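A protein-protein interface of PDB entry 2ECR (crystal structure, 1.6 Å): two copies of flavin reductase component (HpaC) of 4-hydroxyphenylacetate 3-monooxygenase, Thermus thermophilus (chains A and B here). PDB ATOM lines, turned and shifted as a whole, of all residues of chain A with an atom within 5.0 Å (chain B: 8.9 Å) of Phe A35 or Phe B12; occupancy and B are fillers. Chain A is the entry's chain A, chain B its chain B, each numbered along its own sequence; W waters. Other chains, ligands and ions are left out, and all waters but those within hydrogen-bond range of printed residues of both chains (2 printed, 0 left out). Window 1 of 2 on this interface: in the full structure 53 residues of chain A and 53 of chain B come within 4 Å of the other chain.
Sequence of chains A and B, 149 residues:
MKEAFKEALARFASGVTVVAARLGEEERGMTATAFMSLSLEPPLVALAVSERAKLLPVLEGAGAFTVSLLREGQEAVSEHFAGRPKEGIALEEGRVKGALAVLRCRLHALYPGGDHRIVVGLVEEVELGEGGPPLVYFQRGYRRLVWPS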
ATOM      1  N   SER A  14     -12.174 -27.152 -25.448  1.00  0.00           N
ATOM      2  CA  SER A  14     -11.954 -25.822 -24.904  1.00  0.00           C
ATOM      3  C   SER A  14     -13.169 -24.950 -25.095  1.00  0.00           C
ATOM      4  O   SER A  14     -14.042 -25.246 -25.915  1.00  0.00           O
ATOM      5  CB  SER A  14     -10.771 -25.144 -25.596  1.00  0.00           C
ATOM      6  OG  SER A  14     -11.139 -24.691 -26.892  1.00  0.00           O
ATOM      7  N   GLY A  15     -13.224 -23.872 -24.324  1.00  0.00           N
ATOM      8  CA  GLY A  15     -14.302 -22.923 -24.478  1.00  0.00           C
ATOM      9  C   GLY A  15     -13.921 -22.120 -25.708  1.00  0.00           C
ATOM     10  O   GLY A  15     -12.913 -22.418 -26.356  1.00  0.00           O
ATOM     11  N   VAL A  16     -14.710 -21.107 -26.039  1.00  0.00           N
ATOM     12  CA  VAL A  16     -14.426 -20.281 -27.207  1.00  0.00           C
ATOM     13  C   VAL A  16     -14.478 -18.821 -26.789  1.00  0.00           C
ATOM     14  O   VAL A  16     -15.403 -18.402 -26.096  1.00  0.00           O
ATOM     15  CB  VAL A  16     -15.457 -20.525 -28.331  1.00  0.00           C
ATOM     16  CG1 VAL A  16     -15.115 -19.674 -29.547  1.00  0.00           C
ATOM     17  CG2 VAL A  16     -15.481 -22.006 -28.704  1.00  0.00           C
ATOM     18  N   THR A  17     -13.482 -18.048 -27.206  1.00  0.00           N
ATOM     19  CA  THR A  17     -13.439 -16.639 -26.852  1.00  0.00           C
ATOM     20  C   THR A  17     -13.375 -15.767 -28.084  1.00  0.00           C
ATOM     21  O   THR A  17     -13.139 -16.239 -29.195  1.00  0.00           O
ATOM     22  CB  THR A  17     -12.184 -16.289 -26.008  1.00  0.00           C
ATOM     23  OG1 THR A  17     -11.030 -16.232 -26.862  1.00  0.00           O
ATOM     24  CG2 THR A  17     -11.955 -17.337 -24.922  1.00  0.00           C
ATOM     25  N   THR A  33      -9.610 -20.064 -29.587  1.00  0.00           N
ATOM     26  CA  THR A  33      -9.835 -21.145 -28.644  1.00  0.00           C
ATOM     27  C   THR A  33      -8.555 -21.306 -27.833  1.00  0.00           C
ATOM     28  O   THR A  33      -8.570 -21.904 -26.756  1.00  0.00           O
ATOM     29  CB  THR A  33     -10.154 -22.477 -29.350  1.00  0.00           C
ATOM     30  OG1 THR A  33      -9.209 -22.700 -30.404  1.00  0.00           O
ATOM     31  CG2 THR A  33     -11.565 -22.452 -29.919  1.00  0.00           C
ATOM     32  N   ALA A  34      -7.456 -20.761 -28.355  1.00  0.00           N
ATOM     33  CA  ALA A  34      -6.154 -20.825 -27.684  1.00  0.00           C
ATOM     34  C   ALA A  34      -6.070 -19.737 -26.621  1.00  0.00           C
ATOM     35  O   ALA A  34      -5.503 -18.661 -26.846  1.00  0.00           O
ATOM     36  CB  ALA A  34      -5.025 -20.658 -28.690  1.00  0.00           C
ATOM     37  N   PHE A  35      -6.642 -20.048 -25.465  1.00  0.00           N
ATOM     38  CA  PHE A  35      -6.696 -19.151 -24.317  1.00  0.00           C
ATOM     39  C   PHE A  35      -6.464 -19.983 -23.068  1.00  0.00           C
ATOM     40  O   PHE A  35      -6.898 -21.135 -22.993  1.00  0.00           O
ATOM     41  CB  PHE A  35      -8.087 -18.510 -24.225  1.00  0.00           C
ATOM     42  CG  PHE A  35      -8.358 -17.818 -22.914  1.00  0.00           C
ATOM     43  CD1 PHE A  35      -7.987 -16.495 -22.714  1.00  0.00           C
ATOM     44  CD2 PHE A  35      -8.981 -18.503 -21.872  1.00  0.00           C
ATOM     45  CE1 PHE A  35      -8.232 -15.864 -21.492  1.00  0.00           C
ATOM     46  CE2 PHE A  35      -9.228 -17.880 -20.649  1.00  0.00           C
ATOM     47  CZ  PHE A  35      -8.852 -16.556 -20.459  1.00  0.00           C
ATOM     48  N   MET A  36      -5.778 -19.411 -22.085  1.00  0.00           N
ATOM     49  CA  MET A  36      -5.556 -20.119 -20.834  1.00  0.00           C
ATOM     50  C   MET A  36      -5.246 -19.157 -19.705  1.00  0.00           C
ATOM     51  O   MET A  36      -4.719 -18.067 -19.929  1.00  0.00           O
ATOM     52  CB  MET A  36      -4.418 -21.140 -20.966  1.00  0.00           C
ATOM     53  CG  MET A  36      -3.022 -20.559 -21.151  1.00  0.00           C
ATOM     54  SD  MET A  36      -1.815 -21.902 -21.381  1.00  0.00           S
ATOM     55  CE  MET A  36      -0.294 -20.964 -21.523  1.00  0.00           C
ATOM     56  N   SER A  37      -5.607 -19.556 -18.490  1.00  0.00           N
ATOM     57  CA  SER A  37      -5.323 -18.748 -17.315  1.00  0.00           C
ATOM     58  C   SER A  37      -3.824 -18.902 -17.130  1.00  0.00           C
ATOM     59  O   SER A  37      -3.263 -19.952 -17.452  1.00  0.00           O
ATOM     60  CB  SER A  37      -6.053 -19.308 -16.097  1.00  0.00           C
ATOM     61  OG  SER A  37      -5.672 -20.647 -15.859  1.00  0.00           O
ATOM     62  N   VAL A  45      -3.534 -13.677 -18.100  1.00  0.00           N
ATOM     63  CA  VAL A  45      -4.117 -14.679 -18.981  1.00  0.00           C
ATOM     64  C   VAL A  45      -3.225 -14.726 -20.223  1.00  0.00           C
ATOM     65  O   VAL A  45      -2.535 -13.744 -20.534  1.00  0.00           O
ATOM     66  CB  VAL A  45      -5.575 -14.335 -19.393  1.00  0.00           C
ATOM     67  CG1 VAL A  45      -6.482 -14.368 -18.173  1.00  0.00           C
ATOM     68  CG2 VAL A  45      -5.628 -12.975 -20.061  1.00  0.00           C
ATOM     69  N   ALA A  46      -3.208 -15.864 -20.914  1.00  0.00           N
ATOM     70  CA  ALA A  46      -2.390 -16.012 -22.116  1.00  0.00           C
ATOM     71  C   ALA A  46      -3.240 -16.445 -23.298  1.00  0.00           C
ATOM     72  O   ALA A  46      -4.211 -17.186 -23.139  1.00  0.00           O
ATOM     73  CB  ALA A  46      -1.277 -17.027 -21.882  1.00  0.00           C
ATOM     74  N   LEU A  47      -2.863 -15.966 -24.478  1.00  0.00           N
ATOM     75  CA  LEU A  47      -3.561 -16.278 -25.720  1.00  0.00           C
ATOM     76  C   LEU A  47      -2.560 -16.469 -26.850  1.00  0.00           C
ATOM     77  O   LEU A  47      -1.453 -15.924 -26.812  1.00  0.00           O
ATOM     78  CB  LEU A  47      -4.480 -15.122 -26.116  1.00  0.00           C
ATOM     79  CG  LEU A  47      -5.688 -14.756 -25.263  1.00  0.00           C
ATOM     80  CD1 LEU A  47      -5.986 -13.277 -25.435  1.00  0.00           C
ATOM     81  CD2 LEU A  47      -6.884 -15.600 -25.674  1.00  0.00           C
ATOM     82  N   VAL A  67     -11.326  -9.933 -23.754  1.00  0.00           N
ATOM     83  CA  VAL A  67     -11.516 -11.341 -24.045  1.00  0.00           C
ATOM     84  C   VAL A  67     -12.908 -11.684 -23.542  1.00  0.00           C
ATOM     85  O   VAL A  67     -13.196 -11.544 -22.353  1.00  0.00           O
ATOM     86  CB  VAL A  67     -10.495 -12.226 -23.304  1.00  0.00           C
ATOM     87  CG1 VAL A  67     -10.710 -13.684 -23.675  1.00  0.00           C
ATOM     88  CG2 VAL A  67      -9.080 -11.790 -23.650  1.00  0.00           C
ATOM     89  N   LEU A  69     -15.781 -14.632 -23.127  1.00  0.00           N
ATOM     90  CA  LEU A  69     -15.981 -16.080 -23.100  1.00  0.00           C
ATOM     91  C   LEU A  69     -17.405 -16.353 -23.558  1.00  0.00           C
ATOM     92  O   LEU A  69     -18.355 -15.980 -22.881  1.00  0.00           O
ATOM     93  CB  LEU A  69     -15.766 -16.616 -21.683  1.00  0.00           C
ATOM     94  CG  LEU A  69     -14.319 -16.833 -21.213  1.00  0.00           C
ATOM     95  CD1 LEU A  69     -13.480 -15.613 -21.517  1.00  0.00           C
ATOM     96  CD2 LEU A  69     -14.302 -17.144 -19.716  1.00  0.00           C
ATOM     97  N   LEU A 103     -13.046 -10.184 -19.920  1.00  0.00           N
ATOM     98  CA  LEU A 103     -11.841  -9.763 -19.232  1.00  0.00           C
ATOM     99  C   LEU A 103     -11.294  -8.577 -20.014  1.00  0.00           C
ATOM    100  O   LEU A 103     -11.086  -8.678 -21.225  1.00  0.00           O
ATOM    101  CB  LEU A 103     -10.795 -10.885 -19.219  1.00  0.00           C
ATOM    102  CG  LEU A 103     -11.168 -12.197 -18.529  1.00  0.00           C
ATOM    103  CD1 LEU A 103      -9.991 -13.158 -18.610  1.00  0.00           C
ATOM    104  CD2 LEU A 103     -11.528 -11.937 -17.073  1.00  0.00           C
ATOM    105  N   PHE B   5     -12.244 -12.423 -10.965  1.00  0.00           N
ATOM    106  CA  PHE B   5     -11.319 -12.987 -11.942  1.00  0.00           C
ATOM    107  C   PHE B   5     -11.370 -14.510 -11.883  1.00  0.00           C
ATOM    108  O   PHE B   5     -11.453 -15.174 -12.916  1.00  0.00           O
ATOM    109  CB  PHE B   5      -9.896 -12.488 -11.660  1.00  0.00           C
ATOM    110  CG  PHE B   5      -8.842 -13.101 -12.543  1.00  0.00           C
ATOM    111  CD1 PHE B   5      -8.980 -13.095 -13.929  1.00  0.00           C
ATOM    112  CD2 PHE B   5      -7.695 -13.654 -11.988  1.00  0.00           C
ATOM    113  CE1 PHE B   5      -7.985 -13.632 -14.746  1.00  0.00           C
ATOM    114  CE2 PHE B   5      -6.694 -14.191 -12.797  1.00  0.00           C
ATOM    115  CZ  PHE B   5      -6.839 -14.179 -14.176  1.00  0.00           C
ATOM    116  N   LYS B   6     -11.339 -15.066 -10.673  1.00  0.00           N
ATOM    117  CA  LYS B   6     -11.394 -16.516 -10.518  1.00  0.00           C
ATOM    118  C   LYS B   6     -12.696 -17.075 -11.085  1.00  0.00           C
ATOM    119  O   LYS B   6     -12.706 -18.145 -11.692  1.00  0.00           O
ATOM    120  CB  LYS B   6     -11.258 -16.903  -9.042  1.00  0.00           C
ATOM    121  CG  LYS B   6      -9.887 -16.625  -8.445  1.00  0.00           C
ATOM    122  CD  LYS B   6      -9.868 -16.978  -6.966  1.00  0.00           C
ATOM    123  CE  LYS B   6      -8.537 -16.643  -6.319  1.00  0.00           C
ATOM    124  NZ  LYS B   6      -8.599 -16.856  -4.841  1.00  0.00           N
ATOM    125  N   GLU B   7     -13.797 -16.352 -10.891  1.00  0.00           N
ATOM    126  CA  GLU B   7     -15.086 -16.805 -11.397  1.00  0.00           C
ATOM    127  C   GLU B   7     -15.073 -16.787 -12.922  1.00  0.00           C
ATOM    128  O   GLU B   7     -15.625 -17.674 -13.564  1.00  0.00           O
ATOM    129  CB  GLU B   7     -16.213 -15.912 -10.864  1.00  0.00           C
ATOM    130  CG  GLU B   7     -17.609 -16.267 -11.374  1.00  0.00           C
ATOM    131  CD  GLU B   7     -17.988 -17.722 -11.138  1.00  0.00           C
ATOM    132  OE1 GLU B   7     -17.596 -18.282 -10.095  1.00  0.00           O
ATOM    133  OE2 GLU B   7     -18.695 -18.302 -11.992  1.00  0.00           O
ATOM    134  N   ALA B   8     -14.433 -15.777 -13.500  1.00  0.00           N
ATOM    135  CA  ALA B   8     -14.360 -15.686 -14.952  1.00  0.00           C
ATOM    136  C   ALA B   8     -13.595 -16.890 -15.490  1.00  0.00           C
ATOM    137  O   ALA B   8     -13.996 -17.502 -16.475  1.00  0.00           O
ATOM    138  CB  ALA B   8     -13.668 -14.395 -15.366  1.00  0.00           C
ATOM    139  N   LEU B   9     -12.491 -17.229 -14.835  1.00  0.00           N
ATOM    140  CA  LEU B   9     -11.687 -18.367 -15.266  1.00  0.00           C
ATOM    141  C   LEU B   9     -12.456 -19.666 -15.081  1.00  0.00           C
ATOM    142  O   LEU B   9     -12.272 -20.616 -15.840  1.00  0.00           O
ATOM    143  CB  LEU B   9     -10.382 -18.430 -14.478  1.00  0.00           C
ATOM    144  CG  LEU B   9      -9.418 -17.266 -14.701  1.00  0.00           C
ATOM    145  CD1 LEU B   9      -8.166 -17.480 -13.873  1.00  0.00           C
ATOM    146  CD2 LEU B   9      -9.074 -17.160 -16.183  1.00  0.00           C
ATOM    147  N   ALA B  10     -13.307 -19.711 -14.062  1.00  0.00           N
ATOM    148  CA  ALA B  10     -14.111 -20.900 -13.796  1.00  0.00           C
ATOM    149  C   ALA B  10     -15.163 -21.071 -14.890  1.00  0.00           C
ATOM    150  O   ALA B  10     -15.829 -22.107 -14.971  1.00  0.00           O
ATOM    151  CB  ALA B  10     -14.787 -20.788 -12.431  1.00  0.00           C
ATOM    152  N   ARG B  11     -15.310 -20.054 -15.732  1.00  0.00           N
ATOM    153  CA  ARG B  11     -16.280 -20.108 -16.811  1.00  0.00           C
ATOM    154  C   ARG B  11     -15.644 -20.457 -18.150  1.00  0.00           C
ATOM    155  O   ARG B  11     -16.309 -20.420 -19.188  1.00  0.00           O
ATOM    156  CB  ARG B  11     -17.061 -18.792 -16.890  1.00  0.00           C
ATOM    157  CG  ARG B  11     -17.947 -18.597 -15.665  1.00  0.00           C
ATOM    158  CD  ARG B  11     -18.803 -17.345 -15.730  1.00  0.00           C
ATOM    159  NE  ARG B  11     -19.527 -17.151 -14.475  1.00  0.00           N
ATOM    160  CZ  ARG B  11     -20.504 -16.271 -14.299  1.00  0.00           C
ATOM    161  NH1 ARG B  11     -20.887 -15.492 -15.304  1.00  0.00           N
ATOM    162  NH2 ARG B  11     -21.097 -16.171 -13.114  1.00  0.00           N
ATOM    163  N   PHE B  12     -14.352 -20.782 -18.134  1.00  0.00           N
ATOM    164  CA  PHE B  12     -13.685 -21.195 -19.366  1.00  0.00           C
ATOM    165  C   PHE B  12     -13.504 -22.704 -19.286  1.00  0.00           C
ATOM    166  O   PHE B  12     -12.678 -23.203 -18.510  1.00  0.00           O
ATOM    167  CB  PHE B  12     -12.306 -20.543 -19.548  1.00  0.00           C
ATOM    168  CG  PHE B  12     -11.665 -20.872 -20.875  1.00  0.00           C
ATOM    169  CD1 PHE B  12     -12.171 -20.332 -22.055  1.00  0.00           C
ATOM    170  CD2 PHE B  12     -10.595 -21.761 -20.951  1.00  0.00           C
ATOM    171  CE1 PHE B  12     -11.629 -20.671 -23.292  1.00  0.00           C
ATOM    172  CE2 PHE B  12     -10.043 -22.110 -22.190  1.00  0.00           C
ATOM    173  CZ  PHE B  12     -10.561 -21.564 -23.359  1.00  0.00           C
ATOM    174  N   ALA B  13     -14.284 -23.431 -20.080  1.00  0.00           N
ATOM    175  CA  ALA B  13     -14.196 -24.883 -20.099  1.00  0.00           C
ATOM    176  C   ALA B  13     -12.907 -25.299 -20.784  1.00  0.00           C
ATOM    177  O   ALA B  13     -12.413 -24.610 -21.676  1.00  0.00           O
ATOM    178  CB  ALA B  13     -15.383 -25.469 -20.848  1.00  0.00           C
ATOM    179  N   SER B  14     -12.357 -26.430 -20.365  1.00  0.00           N
ATOM    180  CA  SER B  14     -11.138 -26.925 -20.982  1.00  0.00           C
ATOM    181  C   SER B  14     -10.974 -28.406 -20.729  1.00  0.00           C
ATOM    182  O   SER B  14     -11.582 -28.970 -19.818  1.00  0.00           O
ATOM    183  CB  SER B  14      -9.916 -26.211 -20.412  1.00  0.00           C
ATOM    184  OG  SER B  14      -9.634 -26.696 -19.109  1.00  0.00           O
ATOM    185  N   GLY B  15     -10.155 -29.037 -21.557  1.00  0.00           N
ATOM    186  CA  GLY B  15      -9.877 -30.437 -21.352  1.00  0.00           C
ATOM    187  C   GLY B  15      -8.921 -30.464 -20.180  1.00  0.00           C
ATOM    188  O   GLY B  15      -8.583 -29.419 -19.614  1.00  0.00           O
ATOM    189  N   THR B  33      -4.794 -27.732 -16.614  1.00  0.00           N
ATOM    190  CA  THR B  33      -5.878 -27.372 -17.513  1.00  0.00           C
ATOM    191  C   THR B  33      -5.378 -26.230 -18.386  1.00  0.00           C
ATOM    192  O   THR B  33      -5.929 -25.973 -19.453  1.00  0.00           O
ATOM    193  CB  THR B  33      -7.130 -26.891 -16.762  1.00  0.00           C
ATOM    194  OG1 THR B  33      -6.755 -25.922 -15.775  1.00  0.00           O
ATOM    195  CG2 THR B  33      -7.842 -28.067 -16.108  1.00  0.00           C
ATOM    196  N   ALA B  34      -4.330 -25.549 -17.926  1.00  0.00           N
ATOM    197  CA  ALA B  34      -3.751 -24.435 -18.675  1.00  0.00           C
ATOM    198  C   ALA B  34      -2.828 -24.966 -19.764  1.00  0.00           C
ATOM    199  O   ALA B  34      -1.608 -25.032 -19.600  1.00  0.00           O
ATOM    200  CB  ALA B  34      -2.978 -23.508 -17.740  1.00  0.00           C
ATOM    201  N   PHE B  35      -3.436 -25.349 -20.877  1.00  0.00           N
ATOM    202  CA  PHE B  35      -2.728 -25.882 -22.028  1.00  0.00           C
ATOM    203  C   PHE B  35      -3.390 -25.301 -23.267  1.00  0.00           C
ATOM    204  O   PHE B  35      -4.604 -25.115 -23.289  1.00  0.00           O
ATOM    205  CB  PHE B  35      -2.863 -27.408 -22.066  1.00  0.00           C
ATOM    206  CG  PHE B  35      -2.529 -28.013 -23.403  1.00  0.00           C
ATOM    207  CD1 PHE B  35      -1.221 -28.366 -23.718  1.00  0.00           C
ATOM    208  CD2 PHE B  35      -3.518 -28.185 -24.365  1.00  0.00           C
ATOM    209  CE1 PHE B  35      -0.904 -28.879 -24.976  1.00  0.00           C
ATOM    210  CE2 PHE B  35      -3.212 -28.699 -25.628  1.00  0.00           C
ATOM    211  CZ  PHE B  35      -1.900 -29.045 -25.932  1.00  0.00           C
ATOM    212  N   MET B  36      -2.605 -25.014 -24.297  1.00  0.00           N
ATOM    213  CA  MET B  36      -3.185 -24.501 -25.527  1.00  0.00           C
ATOM    214  C   MET B  36      -2.273 -24.762 -26.706  1.00  0.00           C
ATOM    215  O   MET B  36      -1.055 -24.859 -26.552  1.00  0.00           O
ATOM    216  CB  MET B  36      -3.474 -22.998 -25.420  1.00  0.00           C
ATOM    217  CG  MET B  36      -2.254 -22.099 -25.354  1.00  0.00           C
ATOM    218  SD  MET B  36      -2.756 -20.372 -25.114  1.00  0.00           S
ATOM    219  CE  MET B  36      -1.167 -19.530 -25.219  1.00  0.00           C
ATOM    220  N   SER B  37      -2.868 -24.904 -27.885  1.00  0.00           N
ATOM    221  CA  SER B  37      -2.078 -25.108 -29.084  1.00  0.00           C
ATOM    222  C   SER B  37      -1.452 -23.751 -29.342  1.00  0.00           C
ATOM    223  O   SER B  37      -1.998 -22.723 -28.936  1.00  0.00           O
ATOM    224  CB  SER B  37      -2.972 -25.518 -30.256  1.00  0.00           C
ATOM    225  OG  SER B  37      -3.910 -24.508 -30.561  1.00  0.00           O
ATOM    226  N   LEU B  38      -0.311 -23.735 -30.012  1.00  0.00           N
ATOM    227  CA  LEU B  38       0.352 -22.473 -30.275  1.00  0.00           C
ATOM    228  C   LEU B  38       0.718 -22.259 -31.730  1.00  0.00           C
ATOM    229  O   LEU B  38       0.385 -21.227 -32.305  1.00  0.00           O
ATOM    230  CB  LEU B  38       1.608 -22.353 -29.404  1.00  0.00           C
ATOM    231  CG  LEU B  38       2.446 -21.084 -29.603  1.00  0.00           C
ATOM    232  CD1 LEU B  38       1.586 -19.840 -29.368  1.00  0.00           C
ATOM    233  CD2 LEU B  38       3.626 -21.108 -28.641  1.00  0.00           C
ATOM    234  N   ALA B  46       1.726 -24.656 -25.753  1.00  0.00           N
ATOM    235  CA  ALA B  46       2.142 -23.894 -24.586  1.00  0.00           C
ATOM    236  C   ALA B  46       1.312 -24.302 -23.387  1.00  0.00           C
ATOM    237  O   ALA B  46       0.188 -24.773 -23.525  1.00  0.00           O
ATOM    238  CB  ALA B  46       1.978 -22.401 -24.844  1.00  0.00           C
ATOM    239  N   VAL B 136     -13.530 -33.006 -19.074  1.00  0.00           N
ATOM    240  CA  VAL B 136     -13.641 -31.554 -19.138  1.00  0.00           C
ATOM    241  C   VAL B 136     -13.711 -30.957 -17.744  1.00  0.00           C
ATOM    242  O   VAL B 136     -14.220 -31.586 -16.817  1.00  0.00           O
ATOM    243  CB  VAL B 136     -14.913 -31.119 -19.920  1.00  0.00           C
ATOM    244  CG1 VAL B 136     -15.012 -29.597 -19.972  1.00  0.00           C
ATOM    245  CG2 VAL B 136     -14.875 -31.688 -21.330  1.00  0.00           C
ATOM    246  N   TYR B 137     -13.169 -29.754 -17.594  1.00  0.00           N
ATOM    247  CA  TYR B 137     -13.217 -29.064 -16.313  1.00  0.00           C
ATOM    248  C   TYR B 137     -13.916 -27.733 -16.553  1.00  0.00           C
ATOM    249  O   TYR B 137     -13.531 -26.965 -17.435  1.00  0.00           O
ATOM    250  CB  TYR B 137     -11.812 -28.834 -15.754  1.00  0.00           C
ATOM    251  CG  TYR B 137     -11.810 -28.585 -14.258  1.00  0.00           C
ATOM    252  CD1 TYR B 137     -12.077 -29.621 -13.360  1.00  0.00           C
ATOM    253  CD2 TYR B 137     -11.565 -27.314 -13.741  1.00  0.00           C
ATOM    254  CE1 TYR B 137     -12.105 -29.398 -11.984  1.00  0.00           C
ATOM    255  CE2 TYR B 137     -11.591 -27.078 -12.362  1.00  0.00           C
ATOM    256  CZ  TYR B 137     -11.862 -28.124 -11.493  1.00  0.00           C
ATOM    257  OH  TYR B 137     -11.896 -27.901 -10.133  1.00  0.00           O
ATOM    258  N   PHE B 138     -14.952 -27.467 -15.769  1.00  0.00           N
ATOM    259  CA  PHE B 138     -15.725 -26.241 -15.905  1.00  0.00           C
ATOM    260  C   PHE B 138     -16.448 -25.998 -14.589  1.00  0.00           C
ATOM    261  O   PHE B 138     -16.977 -26.932 -13.988  1.00  0.00           O
ATOM    262  CB  PHE B 138     -16.744 -26.402 -17.036  1.00  0.00           C
ATOM    263  CG  PHE B 138     -17.671 -25.228 -17.206  1.00  0.00           C
ATOM    264  CD1 PHE B 138     -17.227 -24.049 -17.799  1.00  0.00           C
ATOM    265  CD2 PHE B 138     -19.003 -25.316 -16.807  1.00  0.00           C
ATOM    266  CE1 PHE B 138     -18.100 -22.974 -17.997  1.00  0.00           C
ATOM    267  CE2 PHE B 138     -19.883 -24.251 -16.998  1.00  0.00           C
ATOM    268  CZ  PHE B 138     -19.430 -23.079 -17.596  1.00  0.00           C
ATOM    269  N   GLN B 139     -16.468 -24.751 -14.141  1.00  0.00           N
ATOM    270  CA  GLN B 139     -17.135 -24.413 -12.890  1.00  0.00           C
ATOM    271  C   GLN B 139     -16.701 -25.280 -11.708  1.00  0.00           C
ATOM    272  O   GLN B 139     -17.531 -25.859 -10.996  1.00  0.00           O
ATOM    273  CB  GLN B 139     -18.652 -24.483 -13.071  1.00  0.00           C
ATOM    274  CG  GLN B 139     -19.231 -23.272 -13.773  1.00  0.00           C
ATOM    275  CD  GLN B 139     -19.165 -22.023 -12.917  1.00  0.00           C
ATOM    276  OE1 GLN B 139     -19.752 -21.971 -11.839  1.00  0.00           O
ATOM    277  NE2 GLN B 139     -18.449 -21.011 -13.391  1.00  0.00           N
ATOM    278  N   ARG B 140     -15.387 -25.366 -11.523  1.00  0.00           N
ATOM    279  CA  ARG B 140     -14.772 -26.097 -10.418  1.00  0.00           C
ATOM    280  C   ARG B 140     -15.172 -27.564 -10.274  1.00  0.00           C
ATOM    281  O   ARG B 140     -15.294 -28.078  -9.161  1.00  0.00           O
ATOM    282  CB  ARG B 140     -15.049 -25.339  -9.112  1.00  0.00           C
ATOM    283  CG  ARG B 140     -14.723 -23.844  -9.204  1.00  0.00           C
ATOM    284  CD  ARG B 140     -15.050 -23.093  -7.918  1.00  0.00           C
ATOM    285  NE  ARG B 140     -14.700 -21.674  -8.010  1.00  0.00           N
ATOM    286  CZ  ARG B 140     -15.400 -20.763  -8.680  1.00  0.00           C
ATOM    287  NH1 ARG B 140     -16.506 -21.107  -9.326  1.00  0.00           N
ATOM    288  NH2 ARG B 140     -14.989 -19.503  -8.707  1.00  0.00           N
ATOM    289  N   GLY B 141     -15.357 -28.245 -11.398  1.00  0.00           N
ATOM    290  CA  GLY B 141     -15.728 -29.646 -11.345  1.00  0.00           C
ATOM    291  C   GLY B 141     -15.531 -30.337 -12.676  1.00  0.00           C
ATOM    292  O   GLY B 141     -15.428 -29.684 -13.716  1.00  0.00           O
HETATM  293  O   HOH W   1      -6.883 -23.738 -23.063  1.00  0.00           O
HETATM  294  O   HOH W   2      -6.266 -23.297 -16.331  1.00  0.00           O
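The side-chain sulfur of Met B36 lies close to the backbone carbonyl oxygen of Ala A34. The backbone carbonyl oxygen (O) of Ala B13 is in hydrogen-bond range of the backbone NH (N) of Gly A15, at 2.9 Å. The side-chain sulfur (SD) of Met A36 sits close to the backbone carbonyl oxygen (O) of Ala B34, at 3.6 Å.
O of Met B36 lies within hydrogen-bond range of N of Ala B46, 2.9 Å away. N of Ala A46 lies within hydrogen-bond range of O of Met A36. OE2 of Glu B7 is in salt-bridge range of NE of Arg B11 (2.9 Å). The backbone NH (N) of Leu A103 is in hydrogen-bond range of the backbone carbonyl oxygen (O) of Val A67, 2.8 Å away.
Among the printed residues, merely in contact across the chains: Leu A69 with Ala B8 (3.3 Å), Phe A35 with Phe B12 (3.4 Å), Ser A14 with Ala B13 (3.5 Å), Ser A37 with Leu B9 (3.6 Å), Ser A37 with Ala B34 (3.6 Å), Gly A15 with Phe B12 (3.6 Å), Ala A34 with Ser B37 (3.7 Å), Leu A103 with Ala B8 (3.7 Å), Thr A17 with Phe B12 (3.7 Å), Leu A47 with Met B36 (3.7 Å), Val A45 with Phe B5 (3.8 Å), Met A36 with Phe B35 (3.8 Å), Leu A69 with Arg B11 (3.9 Å), Phe A35 with Met B36 (3.9 Å), Leu A69 with Phe B12 (3.9 Å), Thr A33 with Phe B12 (3.95 Å) and Met A36 with Met B36 (3.98 Å).
Phe A35 touches just these residues of chain B: Phe B12 and Met B36. Phe B12 touches five residues of chain A. Of chain B, only Phe B12 and Ala B13 come within 4 Å of Gly A15. Printed residues of chain A within 4 Å of Met B36: Ala A34 (3.7 Å), Phe A35 (3.9 Å), Met A36 (3.98 Å) and Leu A47 (3.7 Å). Printed residues of chain B within 4 Å of Leu A103: Ala B8 (3.7 Å). Printed residues of chain B within 4 Å of Thr A33: Phe B12 (3.95 Å). Of the printed residues of chain B, Ser A14 touches Ala B13 (3.5 Å). The nearest residue of chain A that does not touch Phe B12 is Val A16 (4.2 Å). The nearest printed residue of chain B that does not touch Leu A47 is Leu B38 (5.6 Å).
Hydrophobic or aromatic side chains of chain A that line the printed part of chain B: Ala A34, Phe A35, Met A36, Val A45, Leu A69 and Leu A103. Among the printed residues, 20 pairs touch across the chains.
Ala A34 touches Met B36, and with the chains exchanged Met A36 touches Ala B34. Ala A34 touches Ser B37, and with the chains exchanged Ser A37 touches Ala B34. Phe A35 touches Met B36, and with the chains exchanged Met A36 touches Phe B35. Met A36 touches its own counterpart, Met B36. Positions printed for both chains: 14, 15, 33, 34, 35, 36, 37 and 46. Of the 20 pairs that touch across the chains among the printed residues, 7 have their exchanged pair printed and touching as well.
Water W1 lies within hydrogen-bond range of the backbone carbonyl oxygen of Phe A35 and the backbone carbonyl oxygen of Phe B35. Water W2 lies within hydrogen-bond range of the side-chain hydroxyl of Thr B33 (2.7 Å), the side-chain hydroxyl of Ser A37 (2.8 Å) and the backbone NH of Ala B34 (3.4 Å).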
